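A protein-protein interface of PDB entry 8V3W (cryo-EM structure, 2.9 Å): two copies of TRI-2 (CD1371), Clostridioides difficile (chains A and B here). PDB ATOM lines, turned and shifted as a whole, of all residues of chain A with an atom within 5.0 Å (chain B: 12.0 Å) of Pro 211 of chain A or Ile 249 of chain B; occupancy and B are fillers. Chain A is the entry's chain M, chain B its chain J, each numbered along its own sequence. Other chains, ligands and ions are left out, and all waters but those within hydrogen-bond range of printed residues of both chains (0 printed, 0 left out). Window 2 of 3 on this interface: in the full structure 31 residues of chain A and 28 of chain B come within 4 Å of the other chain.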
ATOM      1  N   SER A 188      21.178   2.957  14.176  1.00  0.00           N
ATOM      2  CA  SER A 188      19.767   2.759  13.886  1.00  0.00           C
ATOM      3  C   SER A 188      18.894   2.789  15.130  1.00  0.00           C
ATOM      4  O   SER A 188      17.664   2.764  15.001  1.00  0.00           O
ATOM      5  CB  SER A 188      19.563   1.426  13.159  1.00  0.00           C
ATOM      6  OG  SER A 188      19.954   0.336  13.975  1.00  0.00           O
ATOM      7  N   GLY A 189      19.487   2.854  16.319  1.00  0.00           N
ATOM      8  CA  GLY A 189      18.736   2.588  17.529  1.00  0.00           C
ATOM      9  C   GLY A 189      17.709   3.619  17.945  1.00  0.00           C
ATOM     10  O   GLY A 189      16.510   3.403  17.746  1.00  0.00           O
ATOM     11  N   ASN A 190      18.146   4.764  18.459  1.00  0.00           N
ATOM     12  CA  ASN A 190      17.192   5.642  19.118  1.00  0.00           C
ATOM     13  C   ASN A 190      16.298   6.329  18.090  1.00  0.00           C
ATOM     14  O   ASN A 190      16.592   6.372  16.891  1.00  0.00           O
ATOM     15  CB  ASN A 190      17.910   6.661  20.014  1.00  0.00           C
ATOM     16  CG  ASN A 190      18.782   7.642  19.243  1.00  0.00           C
ATOM     17  OD1 ASN A 190      18.361   8.232  18.249  1.00  0.00           O
ATOM     18  ND2 ASN A 190      20.014   7.816  19.706  1.00  0.00           N
ATOM     19  N   LYS A 191      15.175   6.855  18.576  1.00  0.00           N
ATOM     20  CA  LYS A 191      14.214   7.517  17.708  1.00  0.00           C
ATOM     21  C   LYS A 191      14.704   8.873  17.218  1.00  0.00           C
ATOM     22  O   LYS A 191      14.111   9.426  16.286  1.00  0.00           O
ATOM     23  CB  LYS A 191      12.887   7.673  18.451  1.00  0.00           C
ATOM     24  CG  LYS A 191      11.668   7.824  17.563  1.00  0.00           C
ATOM     25  CD  LYS A 191      10.400   7.741  18.393  1.00  0.00           C
ATOM     26  CE  LYS A 191       9.166   8.007  17.558  1.00  0.00           C
ATOM     27  NZ  LYS A 191       7.944   8.088  18.400  1.00  0.00           N
ATOM     28  N   TYR A 194      15.480   9.890  13.329  1.00  0.00           N
ATOM     29  CA  TYR A 194      14.419  10.212  12.382  1.00  0.00           C
ATOM     30  C   TYR A 194      14.074  11.694  12.420  1.00  0.00           C
ATOM     31  O   TYR A 194      13.979  12.346  11.372  1.00  0.00           O
ATOM     32  CB  TYR A 194      13.191   9.352  12.669  1.00  0.00           C
ATOM     33  CG  TYR A 194      13.401   7.911  12.287  1.00  0.00           C
ATOM     34  CD1 TYR A 194      13.136   7.471  10.997  1.00  0.00           C
ATOM     35  CD2 TYR A 194      13.881   6.992  13.209  1.00  0.00           C
ATOM     36  CE1 TYR A 194      13.335   6.156  10.639  1.00  0.00           C
ATOM     37  CE2 TYR A 194      14.082   5.674  12.861  1.00  0.00           C
ATOM     38  CZ  TYR A 194      13.807   5.260  11.574  1.00  0.00           C
ATOM     39  OH  TYR A 194      14.006   3.947  11.223  1.00  0.00           O
ATOM     40  N   VAL A 209       6.951  11.643  14.971  1.00  0.00           N
ATOM     41  CA  VAL A 209       7.157  10.314  14.406  1.00  0.00           C
ATOM     42  C   VAL A 209       6.255   9.327  15.133  1.00  0.00           C
ATOM     43  O   VAL A 209       6.178   9.341  16.366  1.00  0.00           O
ATOM     44  CB  VAL A 209       8.629   9.871  14.502  1.00  0.00           C
ATOM     45  CG1 VAL A 209       8.801   8.473  13.927  1.00  0.00           C
ATOM     46  CG2 VAL A 209       9.529  10.858  13.783  1.00  0.00           C
ATOM     47  N   TYR A 210       5.574   8.476  14.369  1.00  0.00           N
ATOM     48  CA  TYR A 210       4.660   7.477  14.921  1.00  0.00           C
ATOM     49  C   TYR A 210       5.174   6.080  14.614  1.00  0.00           C
ATOM     50  O   TYR A 210       5.051   5.606  13.470  1.00  0.00           O
ATOM     51  CB  TYR A 210       3.254   7.670  14.360  1.00  0.00           C
ATOM     52  CG  TYR A 210       2.670   9.024  14.684  1.00  0.00           C
ATOM     53  CD1 TYR A 210       2.179   9.304  15.951  1.00  0.00           C
ATOM     54  CD2 TYR A 210       2.622  10.025  13.726  1.00  0.00           C
ATOM     55  CE1 TYR A 210       1.651  10.542  16.251  1.00  0.00           C
ATOM     56  CE2 TYR A 210       2.095  11.264  14.017  1.00  0.00           C
ATOM     57  CZ  TYR A 210       1.611  11.519  15.281  1.00  0.00           C
ATOM     58  OH  TYR A 210       1.085  12.756  15.572  1.00  0.00           O
ATOM     59  N   PRO A 211       5.757   5.386  15.586  1.00  0.00           N
ATOM     60  CA  PRO A 211       6.217   4.016  15.341  1.00  0.00           C
ATOM     61  C   PRO A 211       5.053   3.085  15.051  1.00  0.00           C
ATOM     62  O   PRO A 211       3.933   3.290  15.526  1.00  0.00           O
ATOM     63  CB  PRO A 211       6.924   3.632  16.648  1.00  0.00           C
ATOM     64  CG  PRO A 211       7.123   4.924  17.395  1.00  0.00           C
ATOM     65  CD  PRO A 211       6.014   5.823  16.966  1.00  0.00           C
ATOM     66  N   ARG A 212       5.341   2.056  14.249  1.00  0.00           N
ATOM     67  CA  ARG A 212       4.406   0.997  13.869  1.00  0.00           C
ATOM     68  C   ARG A 212       3.011   1.526  13.546  1.00  0.00           C
ATOM     69  O   ARG A 212       2.000   0.934  13.940  1.00  0.00           O
ATOM     70  CB  ARG A 212       4.358  -0.081  14.962  1.00  0.00           C
ATOM     71  CG  ARG A 212       3.751   0.322  16.302  1.00  0.00           C
ATOM     72  CD  ARG A 212       3.886  -0.788  17.335  1.00  0.00           C
ATOM     73  NE  ARG A 212       3.667  -2.118  16.778  1.00  0.00           N
ATOM     74  CZ  ARG A 212       4.636  -2.971  16.470  1.00  0.00           C
ATOM     75  NH1 ARG A 212       5.911  -2.651  16.620  1.00  0.00           N
ATOM     76  NH2 ARG A 212       4.317  -4.171  15.996  1.00  0.00           N
ATOM     77  N   TRP A 213       2.951   2.632  12.801  1.00  0.00           N
ATOM     78  CA  TRP A 213       1.666   3.226  12.444  1.00  0.00           C
ATOM     79  C   TRP A 213       0.841   2.307  11.554  1.00  0.00           C
ATOM     80  O   TRP A 213      -0.394   2.345  11.603  1.00  0.00           O
ATOM     81  CB  TRP A 213       1.886   4.565  11.745  1.00  0.00           C
ATOM     82  CG  TRP A 213       1.865   4.460  10.253  1.00  0.00           C
ATOM     83  CD1 TRP A 213       2.895   4.079   9.446  1.00  0.00           C
ATOM     84  CD2 TRP A 213       0.760   4.742   9.387  1.00  0.00           C
ATOM     85  NE1 TRP A 213       2.501   4.103   8.131  1.00  0.00           N
ATOM     86  CE2 TRP A 213       1.194   4.507   8.068  1.00  0.00           C
ATOM     87  CE3 TRP A 213      -0.555   5.166   9.599  1.00  0.00           C
ATOM     88  CZ2 TRP A 213       0.362   4.685   6.966  1.00  0.00           C
ATOM     89  CZ3 TRP A 213      -1.379   5.343   8.503  1.00  0.00           C
ATOM     90  CH2 TRP A 213      -0.918   5.103   7.204  1.00  0.00           C
ATOM     91  N   THR A 218       6.840  -0.411  10.029  1.00  0.00           N
ATOM     92  CA  THR A 218       6.253   0.789   9.448  1.00  0.00           C
ATOM     93  C   THR A 218       6.523   1.989  10.345  1.00  0.00           C
ATOM     94  O   THR A 218       6.437   1.891  11.572  1.00  0.00           O
ATOM     95  CB  THR A 218       4.743   0.627   9.243  1.00  0.00           C
ATOM     96  OG1 THR A 218       4.097   0.480  10.514  1.00  0.00           O
ATOM     97  CG2 THR A 218       4.447  -0.594   8.385  1.00  0.00           C
ATOM     98  N   VAL A 219       6.861   3.118   9.724  1.00  0.00           N
ATOM     99  CA  VAL A 219       7.137   4.363  10.429  1.00  0.00           C
ATOM    100  C   VAL A 219       6.438   5.498   9.694  1.00  0.00           C
ATOM    101  O   VAL A 219       6.528   5.595   8.464  1.00  0.00           O
ATOM    102  CB  VAL A 219       8.650   4.638  10.540  1.00  0.00           C
ATOM    103  CG1 VAL A 219       8.903   6.035  11.084  1.00  0.00           C
ATOM    104  CG2 VAL A 219       9.316   3.600  11.431  1.00  0.00           C
ATOM    105  N   SER B 188      25.158   0.129  12.862  1.00  0.00           N
ATOM    106  CA  SER B 188      23.759   0.390  13.178  1.00  0.00           C
ATOM    107  C   SER B 188      22.964  -0.889  13.407  1.00  0.00           C
ATOM    108  O   SER B 188      22.696  -1.645  12.467  1.00  0.00           O
ATOM    109  CB  SER B 188      23.113   1.210  12.058  1.00  0.00           C
ATOM    110  OG  SER B 188      23.869   2.376  11.776  1.00  0.00           O
ATOM    111  N   GLY B 189      22.590  -1.134  14.662  1.00  0.00           N
ATOM    112  CA  GLY B 189      21.685  -2.203  15.022  1.00  0.00           C
ATOM    113  C   GLY B 189      22.292  -3.584  15.119  1.00  0.00           C
ATOM    114  O   GLY B 189      21.567  -4.534  15.439  1.00  0.00           O
ATOM    115  N   ASN B 190      23.591  -3.733  14.877  1.00  0.00           N
ATOM    116  CA  ASN B 190      24.174  -5.062  14.790  1.00  0.00           C
ATOM    117  C   ASN B 190      24.239  -5.725  16.164  1.00  0.00           C
ATOM    118  O   ASN B 190      23.994  -5.105  17.204  1.00  0.00           O
ATOM    119  CB  ASN B 190      25.565  -5.000  14.161  1.00  0.00           C
ATOM    120  CG  ASN B 190      26.589  -4.349  15.064  1.00  0.00           C
ATOM    121  OD1 ASN B 190      26.248  -3.595  15.970  1.00  0.00           O
ATOM    122  ND2 ASN B 190      27.860  -4.634  14.812  1.00  0.00           N
ATOM    123  N   HIS B 193      26.277  -3.953  18.558  1.00  0.00           N
ATOM    124  CA  HIS B 193      25.583  -2.829  19.182  1.00  0.00           C
ATOM    125  C   HIS B 193      24.717  -3.289  20.346  1.00  0.00           C
ATOM    126  O   HIS B 193      24.671  -2.628  21.388  1.00  0.00           O
ATOM    127  CB  HIS B 193      24.731  -2.076  18.162  1.00  0.00           C
ATOM    128  CG  HIS B 193      25.382  -0.839  17.627  1.00  0.00           C
ATOM    129  ND1 HIS B 193      24.704   0.090  16.868  1.00  0.00           N
ATOM    130  CD2 HIS B 193      26.650  -0.380  17.740  1.00  0.00           C
ATOM    131  CE1 HIS B 193      25.524   1.074  16.545  1.00  0.00           C
ATOM    132  NE2 HIS B 193      26.712   0.811  17.057  1.00  0.00           N
ATOM    133  N   TYR B 194      24.001  -4.404  20.178  1.00  0.00           N
ATOM    134  CA  TYR B 194      23.226  -4.952  21.288  1.00  0.00           C
ATOM    135  C   TYR B 194      24.128  -5.277  22.469  1.00  0.00           C
ATOM    136  O   TYR B 194      23.807  -4.947  23.618  1.00  0.00           O
ATOM    137  CB  TYR B 194      22.471  -6.204  20.841  1.00  0.00           C
ATOM    138  CG  TYR B 194      21.286  -5.936  19.945  1.00  0.00           C
ATOM    139  CD1 TYR B 194      20.116  -5.396  20.456  1.00  0.00           C
ATOM    140  CD2 TYR B 194      21.336  -6.225  18.592  1.00  0.00           C
ATOM    141  CE1 TYR B 194      19.029  -5.151  19.644  1.00  0.00           C
ATOM    142  CE2 TYR B 194      20.253  -5.980  17.773  1.00  0.00           C
ATOM    143  CZ  TYR B 194      19.102  -5.444  18.302  1.00  0.00           C
ATOM    144  OH  TYR B 194      18.024  -5.202  17.485  1.00  0.00           O
ATOM    145  N   TRP B 197      25.226  -1.900  24.108  1.00  0.00           N
ATOM    146  CA  TRP B 197      24.120  -1.321  24.861  1.00  0.00           C
ATOM    147  C   TRP B 197      23.839  -2.107  26.133  1.00  0.00           C
ATOM    148  O   TRP B 197      23.444  -1.523  27.148  1.00  0.00           O
ATOM    149  CB  TRP B 197      22.864  -1.260  23.991  1.00  0.00           C
ATOM    150  CG  TRP B 197      22.960  -0.281  22.867  1.00  0.00           C
ATOM    151  CD1 TRP B 197      23.515   0.963  22.911  1.00  0.00           C
ATOM    152  CD2 TRP B 197      22.494  -0.465  21.524  1.00  0.00           C
ATOM    153  NE1 TRP B 197      23.420   1.567  21.681  1.00  0.00           N
ATOM    154  CE2 TRP B 197      22.799   0.710  20.812  1.00  0.00           C
ATOM    155  CE3 TRP B 197      21.848  -1.510  20.856  1.00  0.00           C
ATOM    156  CZ2 TRP B 197      22.481   0.871  19.466  1.00  0.00           C
ATOM    157  CZ3 TRP B 197      21.534  -1.350  19.521  1.00  0.00           C
ATOM    158  CH2 TRP B 197      21.849  -0.167  18.840  1.00  0.00           C
ATOM    159  N   PRO B 216      11.820 -13.610  12.700  1.00  0.00           N
ATOM    160  CA  PRO B 216      12.420 -12.317  12.353  1.00  0.00           C
ATOM    161  C   PRO B 216      11.905 -11.201  13.249  1.00  0.00           C
ATOM    162  O   PRO B 216      10.768 -11.226  13.723  1.00  0.00           O
ATOM    163  CB  PRO B 216      11.993 -12.108  10.895  1.00  0.00           C
ATOM    164  CG  PRO B 216      11.547 -13.464  10.415  1.00  0.00           C
ATOM    165  CD  PRO B 216      10.962 -14.121  11.620  1.00  0.00           C
ATOM    166  N   GLY B 217      12.764 -10.213  13.481  1.00  0.00           N
ATOM    167  CA  GLY B 217      12.405  -9.099  14.335  1.00  0.00           C
ATOM    168  C   GLY B 217      12.387  -9.406  15.812  1.00  0.00           C
ATOM    169  O   GLY B 217      11.763  -8.667  16.579  1.00  0.00           O
ATOM    170  N   THR B 218      13.044 -10.480  16.236  1.00  0.00           N
ATOM    171  CA  THR B 218      13.118 -10.855  17.641  1.00  0.00           C
ATOM    172  C   THR B 218      14.575 -11.056  18.025  1.00  0.00           C
ATOM    173  O   THR B 218      15.303 -11.791  17.348  1.00  0.00           O
ATOM    174  CB  THR B 218      12.316 -12.131  17.913  1.00  0.00           C
ATOM    175  OG1 THR B 218      12.751 -13.163  17.021  1.00  0.00           O
ATOM    176  CG2 THR B 218      10.836 -11.881  17.705  1.00  0.00           C
ATOM    177  N   VAL B 219      14.998 -10.408  19.107  1.00  0.00           N
ATOM    178  CA  VAL B 219      16.362 -10.512  19.610  1.00  0.00           C
ATOM    179  C   VAL B 219      16.306 -11.007  21.046  1.00  0.00           C
ATOM    180  O   VAL B 219      15.615 -10.418  21.885  1.00  0.00           O
ATOM    181  CB  VAL B 219      17.106  -9.167  19.524  1.00  0.00           C
ATOM    182  CG1 VAL B 219      18.471  -9.274  20.183  1.00  0.00           C
ATOM    183  CG2 VAL B 219      17.246  -8.733  18.076  1.00  0.00           C
ATOM    184  N   GLN B 240      16.568  -3.861  30.026  1.00  0.00           N
ATOM    185  CA  GLN B 240      15.552  -3.886  28.981  1.00  0.00           C
ATOM    186  C   GLN B 240      15.150  -2.478  28.569  1.00  0.00           C
ATOM    187  O   GLN B 240      15.033  -2.185  27.375  1.00  0.00           O
ATOM    188  CB  GLN B 240      14.332  -4.674  29.457  1.00  0.00           C
ATOM    189  CG  GLN B 240      13.139  -4.594  28.522  1.00  0.00           C
ATOM    190  CD  GLN B 240      13.321  -5.440  27.279  1.00  0.00           C
ATOM    191  OE1 GLN B 240      13.197  -4.950  26.157  1.00  0.00           O
ATOM    192  NE2 GLN B 240      13.623  -6.719  27.473  1.00  0.00           N
ATOM    193  N   GLN B 241      14.934  -1.587  29.536  1.00  0.00           N
ATOM    194  CA  GLN B 241      14.542  -0.230  29.167  1.00  0.00           C
ATOM    195  C   GLN B 241      15.690   0.503  28.484  1.00  0.00           C
ATOM    196  O   GLN B 241      15.465   1.290  27.556  1.00  0.00           O
ATOM    197  CB  GLN B 241      14.036   0.544  30.386  1.00  0.00           C
ATOM    198  CG  GLN B 241      15.017   0.672  31.533  1.00  0.00           C
ATOM    199  CD  GLN B 241      15.934   1.870  31.391  1.00  0.00           C
ATOM    200  OE1 GLN B 241      15.482   2.986  31.142  1.00  0.00           O
ATOM    201  NE2 GLN B 241      17.234   1.640  31.539  1.00  0.00           N
ATOM    202  N   HIS B 242      16.931   0.241  28.904  1.00  0.00           N
ATOM    203  CA  HIS B 242      18.070   0.881  28.257  1.00  0.00           C
ATOM    204  C   HIS B 242      18.200   0.434  26.806  1.00  0.00           C
ATOM    205  O   HIS B 242      18.397   1.259  25.903  1.00  0.00           O
ATOM    206  CB  HIS B 242      19.352   0.582  29.031  1.00  0.00           C
ATOM    207  CG  HIS B 242      20.540   1.350  28.542  1.00  0.00           C
ATOM    208  ND1 HIS B 242      20.612   2.724  28.597  1.00  0.00           N
ATOM    209  CD2 HIS B 242      21.703   0.934  27.986  1.00  0.00           C
ATOM    210  CE1 HIS B 242      21.767   3.123  28.096  1.00  0.00           C
ATOM    211  NE2 HIS B 242      22.448   2.057  27.718  1.00  0.00           N
ATOM    212  N   ILE B 243      18.076  -0.873  26.554  1.00  0.00           N
ATOM    213  CA  ILE B 243      18.180  -1.343  25.177  1.00  0.00           C
ATOM    214  C   ILE B 243      16.995  -0.844  24.359  1.00  0.00           C
ATOM    215  O   ILE B 243      17.153  -0.458  23.199  1.00  0.00           O
ATOM    216  CB  ILE B 243      18.323  -2.877  25.110  1.00  0.00           C
ATOM    217  CG1 ILE B 243      18.343  -3.338  23.655  1.00  0.00           C
ATOM    218  CG2 ILE B 243      17.187  -3.578  25.808  1.00  0.00           C
ATOM    219  CD1 ILE B 243      19.679  -3.164  23.003  1.00  0.00           C
ATOM    220  N   ASP B 244      15.801  -0.803  24.961  1.00  0.00           N
ATOM    221  CA  ASP B 244      14.636  -0.269  24.262  1.00  0.00           C
ATOM    222  C   ASP B 244      14.862   1.177  23.845  1.00  0.00           C
ATOM    223  O   ASP B 244      14.515   1.571  22.726  1.00  0.00           O
ATOM    224  CB  ASP B 244      13.397  -0.381  25.150  1.00  0.00           C
ATOM    225  CG  ASP B 244      12.872  -1.797  25.238  1.00  0.00           C
ATOM    226  OD1 ASP B 244      13.101  -2.578  24.292  1.00  0.00           O
ATOM    227  OD2 ASP B 244      12.243  -2.134  26.262  1.00  0.00           O
ATOM    228  N   GLU B 245      15.446   1.983  24.734  1.00  0.00           N
ATOM    229  CA  GLU B 245      15.838   3.333  24.352  1.00  0.00           C
ATOM    230  C   GLU B 245      16.879   3.316  23.241  1.00  0.00           C
ATOM    231  O   GLU B 245      16.879   4.200  22.378  1.00  0.00           O
ATOM    232  CB  GLU B 245      16.376   4.095  25.564  1.00  0.00           C
ATOM    233  CG  GLU B 245      15.316   4.511  26.574  1.00  0.00           C
ATOM    234  CD  GLU B 245      15.907   5.244  27.766  1.00  0.00           C
ATOM    235  OE1 GLU B 245      17.129   5.505  27.758  1.00  0.00           O
ATOM    236  OE2 GLU B 245      15.152   5.561  28.709  1.00  0.00           O
ATOM    237  N   GLU B 246      17.767   2.322  23.241  1.00  0.00           N
ATOM    238  CA  GLU B 246      18.832   2.242  22.250  1.00  0.00           C
ATOM    239  C   GLU B 246      18.556   1.243  21.131  1.00  0.00           C
ATOM    240  O   GLU B 246      19.391   1.106  20.232  1.00  0.00           O
ATOM    241  CB  GLU B 246      20.160   1.890  22.931  1.00  0.00           C
ATOM    242  CG  GLU B 246      20.591   2.856  24.022  1.00  0.00           C
ATOM    243  CD  GLU B 246      20.926   4.239  23.491  1.00  0.00           C
ATOM    244  OE1 GLU B 246      21.252   4.357  22.291  1.00  0.00           O
ATOM    245  OE2 GLU B 246      20.870   5.207  24.278  1.00  0.00           O
ATOM    246  N   LYS B 247      17.423   0.537  21.160  1.00  0.00           N
ATOM    247  CA  LYS B 247      17.119  -0.387  20.076  1.00  0.00           C
ATOM    248  C   LYS B 247      16.467   0.349  18.910  1.00  0.00           C
ATOM    249  O   LYS B 247      15.792   1.360  19.109  1.00  0.00           O
ATOM    250  CB  LYS B 247      16.190  -1.497  20.557  1.00  0.00           C
ATOM    251  CG  LYS B 247      14.749  -1.051  20.735  1.00  0.00           C
ATOM    252  CD  LYS B 247      13.825  -2.213  21.028  1.00  0.00           C
ATOM    253  CE  LYS B 247      12.398  -1.729  21.218  1.00  0.00           C
ATOM    254  NZ  LYS B 247      11.417  -2.559  20.474  1.00  0.00           N
ATOM    255  N   PRO B 248      16.646  -0.146  17.686  1.00  0.00           N
ATOM    256  CA  PRO B 248      15.951   0.455  16.543  1.00  0.00           C
ATOM    257  C   PRO B 248      14.445   0.288  16.660  1.00  0.00           C
ATOM    258  O   PRO B 248      13.935  -0.559  17.396  1.00  0.00           O
ATOM    259  CB  PRO B 248      16.506  -0.313  15.336  1.00  0.00           C
ATOM    260  CG  PRO B 248      17.149  -1.536  15.903  1.00  0.00           C
ATOM    261  CD  PRO B 248      17.624  -1.162  17.268  1.00  0.00           C
ATOM    262  N   ILE B 249      13.727   1.128  15.922  1.00  0.00           N
ATOM    263  CA  ILE B 249      12.269   1.133  15.966  1.00  0.00           C
ATOM    264  C   ILE B 249      11.743  -0.034  15.138  1.00  0.00           C
ATOM    265  O   ILE B 249      11.995  -0.117  13.932  1.00  0.00           O
ATOM    266  CB  ILE B 249      11.709   2.471  15.462  1.00  0.00           C
ATOM    267  CG1 ILE B 249      12.046   3.592  16.450  1.00  0.00           C
ATOM    268  CG2 ILE B 249      10.214   2.374  15.251  1.00  0.00           C
ATOM    269  CD1 ILE B 249      13.325   4.339  16.131  1.00  0.00           C
ATOM    270  N   GLY B 250      11.013  -0.939  15.790  1.00  0.00           N
ATOM    271  CA  GLY B 250      10.453  -2.096  15.127  1.00  0.00           C
ATOM    272  C   GLY B 250      10.818  -3.435  15.747  1.00  0.00           C
ATOM    273  O   GLY B 250       9.960  -4.312  15.898  1.00  0.00           O
ATOM    274  N   PRO B 251      12.083  -3.631  16.116  1.00  0.00           N
ATOM    275  CA  PRO B 251      12.459  -4.865  16.814  1.00  0.00           C
ATOM    276  C   PRO B 251      11.815  -4.969  18.187  1.00  0.00           C
ATOM    277  O   PRO B 251      11.381  -3.983  18.784  1.00  0.00           O
ATOM    278  CB  PRO B 251      13.982  -4.757  16.936  1.00  0.00           C
ATOM    279  CG  PRO B 251      14.383  -3.911  15.805  1.00  0.00           C
ATOM    280  CD  PRO B 251      13.261  -2.956  15.542  1.00  0.00           C
ATOM    281  N   THR B 252      11.753  -6.204  18.682  1.00  0.00           N
ATOM    282  CA  THR B 252      11.282  -6.503  20.027  1.00  0.00           C
ATOM    283  C   THR B 252      12.366  -7.277  20.765  1.00  0.00           C
ATOM    284  O   THR B 252      12.917  -8.242  20.226  1.00  0.00           O
ATOM    285  CB  THR B 252       9.981  -7.308  19.998  1.00  0.00           C
ATOM    286  OG1 THR B 252       8.998  -6.601  19.232  1.00  0.00           O
ATOM    287  CG2 THR B 252       9.454  -7.518  21.407  1.00  0.00           C
ATOM    288  N   ILE B 253      12.663  -6.858  21.993  1.00  0.00           N
ATOM    289  CA  ILE B 253      13.784  -7.389  22.762  1.00  0.00           C
ATOM    290  C   ILE B 253      13.252  -8.237  23.908  1.00  0.00           C
ATOM    291  O   ILE B 253      12.389  -7.790  24.674  1.00  0.00           O
ATOM    292  CB  ILE B 253      14.685  -6.260  23.291  1.00  0.00           C
ATOM    293  CG1 ILE B 253      15.113  -5.343  22.146  1.00  0.00           C
ATOM    294  CG2 ILE B 253      15.892  -6.837  24.004  1.00  0.00           C
ATOM    295  CD1 ILE B 253      15.791  -6.066  21.007  1.00  0.00           C
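N of Gly 189 of chain B sits at hydrogen-bond distance from OG of Ser 188 of chain A (3.1 Å). The backbone carbonyl oxygen (O) of Lys 247 of chain B lies close to the backbone carbonyl oxygen (O) of Gly 189 of chain A, 2.6 Å away.
A ring nitrogen (ND1) of His 193 of chain B sits at hydrogen-bond distance from the backbone NH (N) of Gly 189 of chain B, 3.3 Å away. The side-chain amino group of Lys 191 of chain A is in hydrogen-bond range of the backbone carbonyl oxygen of Val 209 of chain A (3.0 Å).
Ser 188 of chain B touches Ser 188 of chain A. Ser 188 of chain A touches Pro 248 of chain B. Glu 246 of chain B touches Gly 189 of chain A (O to CA, 3.2 Å). CA of Pro 248 of chain B touches O of Gly 189 of chain A (3.2 Å). O of Gly 189 of chain A touches CD1 of Ile 249 of chain B, at 3.7 Å. Asn 190 of chain A touches Glu 245 of chain B. O of Asn 190 of chain A touches CD1 of Ile 249 of chain B (3.9 Å). Ile 249 of chain B touches Lys 191 of chain A. Tyr 194 of chain A touches Ile 249 of chain B (CE2 to CD1, 3.6 Å). Ile 249 of chain B touches Pro 211 of chain A (CG2 to CB, 3.8 Å).
Gly 189 of chain A touches four residues of chain B. Of the printed residues of chain B, Tyr 194 of chain A touches Ile 249 (3.6 Å). No residue of chain B comes within 4 Å of Val 209 of chain A. Of the printed residues of chain B, Pro 211 of chain A touches Ile 249. Arg 212 of chain A touches none of the printed residues of chain B. No residue of chain B comes within 4 Å of Thr 218 of chain A. No residue of chain B comes within 4 Å of Val 219 of chain A. Of the printed residues of chain A, Gly 189 of chain B touches Ser 188. Of the printed residues of chain A, Glu 245 of chain B touches Asn 190. Of the printed residues of chain A, Glu 246 of chain B touches Gly 189 (3.2 Å). Of the printed residues of chain A, Pro 248 of chain B touches Ser 188 (3.3 Å) and Gly 189 (3.2 Å). Ile 249 of chain B touches just these residues of chain A: Gly 189 (3.7 Å), Asn 190 (3.9 Å), Lys 191 (3.7 Å), Tyr 194 (3.6 Å) and Pro 211 (3.8 Å). The nearest residue of chain A that does not touch Ile 249 of chain B is Val 219 of chain A (4.1 Å). The nearest printed residue of chain B that does not touch Asn 190 of chain A is Lys 247 of chain B (4.2 Å).
Hydrophobic or aromatic side chains of chain A within 4 Å of the printed part of chain B: Tyr 194 and Pro 211. Of the 24 printed residues of chain B, 7 touch a printed residue of chain A. Printed residues of chain B that touch a printed residue of chain A: Ser 188, Gly 189, Glu 245, Glu 246, Lys 247, Pro 248 and Ile 249. Hydrophobic or aromatic side chains of chain B within 4 Å of the printed part of chain A: Pro 248 and Ile 249. Along chain B the printed residues that touch a printed residue of chain A span positions 188 to 249. Among the printed residues, 12 pairs touch across the chains. Among the printed residues, no Asp or Glu carboxylate lies within 4 Å of a Lys or Arg side-chain nitrogen of the other chain.
Ser 188 of chain A touches its own counterpart, Ser 188 of chain B. Ser 188 of chain A touches Gly 189 of chain B, but with the chains exchanged Gly 189 of chain A does not touch Ser 188 of chain B (5.8 Å). Positions printed for both chains: 188, 189, 190, 194, 218 and 219. Of the 12 pairs that touch across the chains among the printed residues, 1 has its exchanged pair printed and touching as well.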
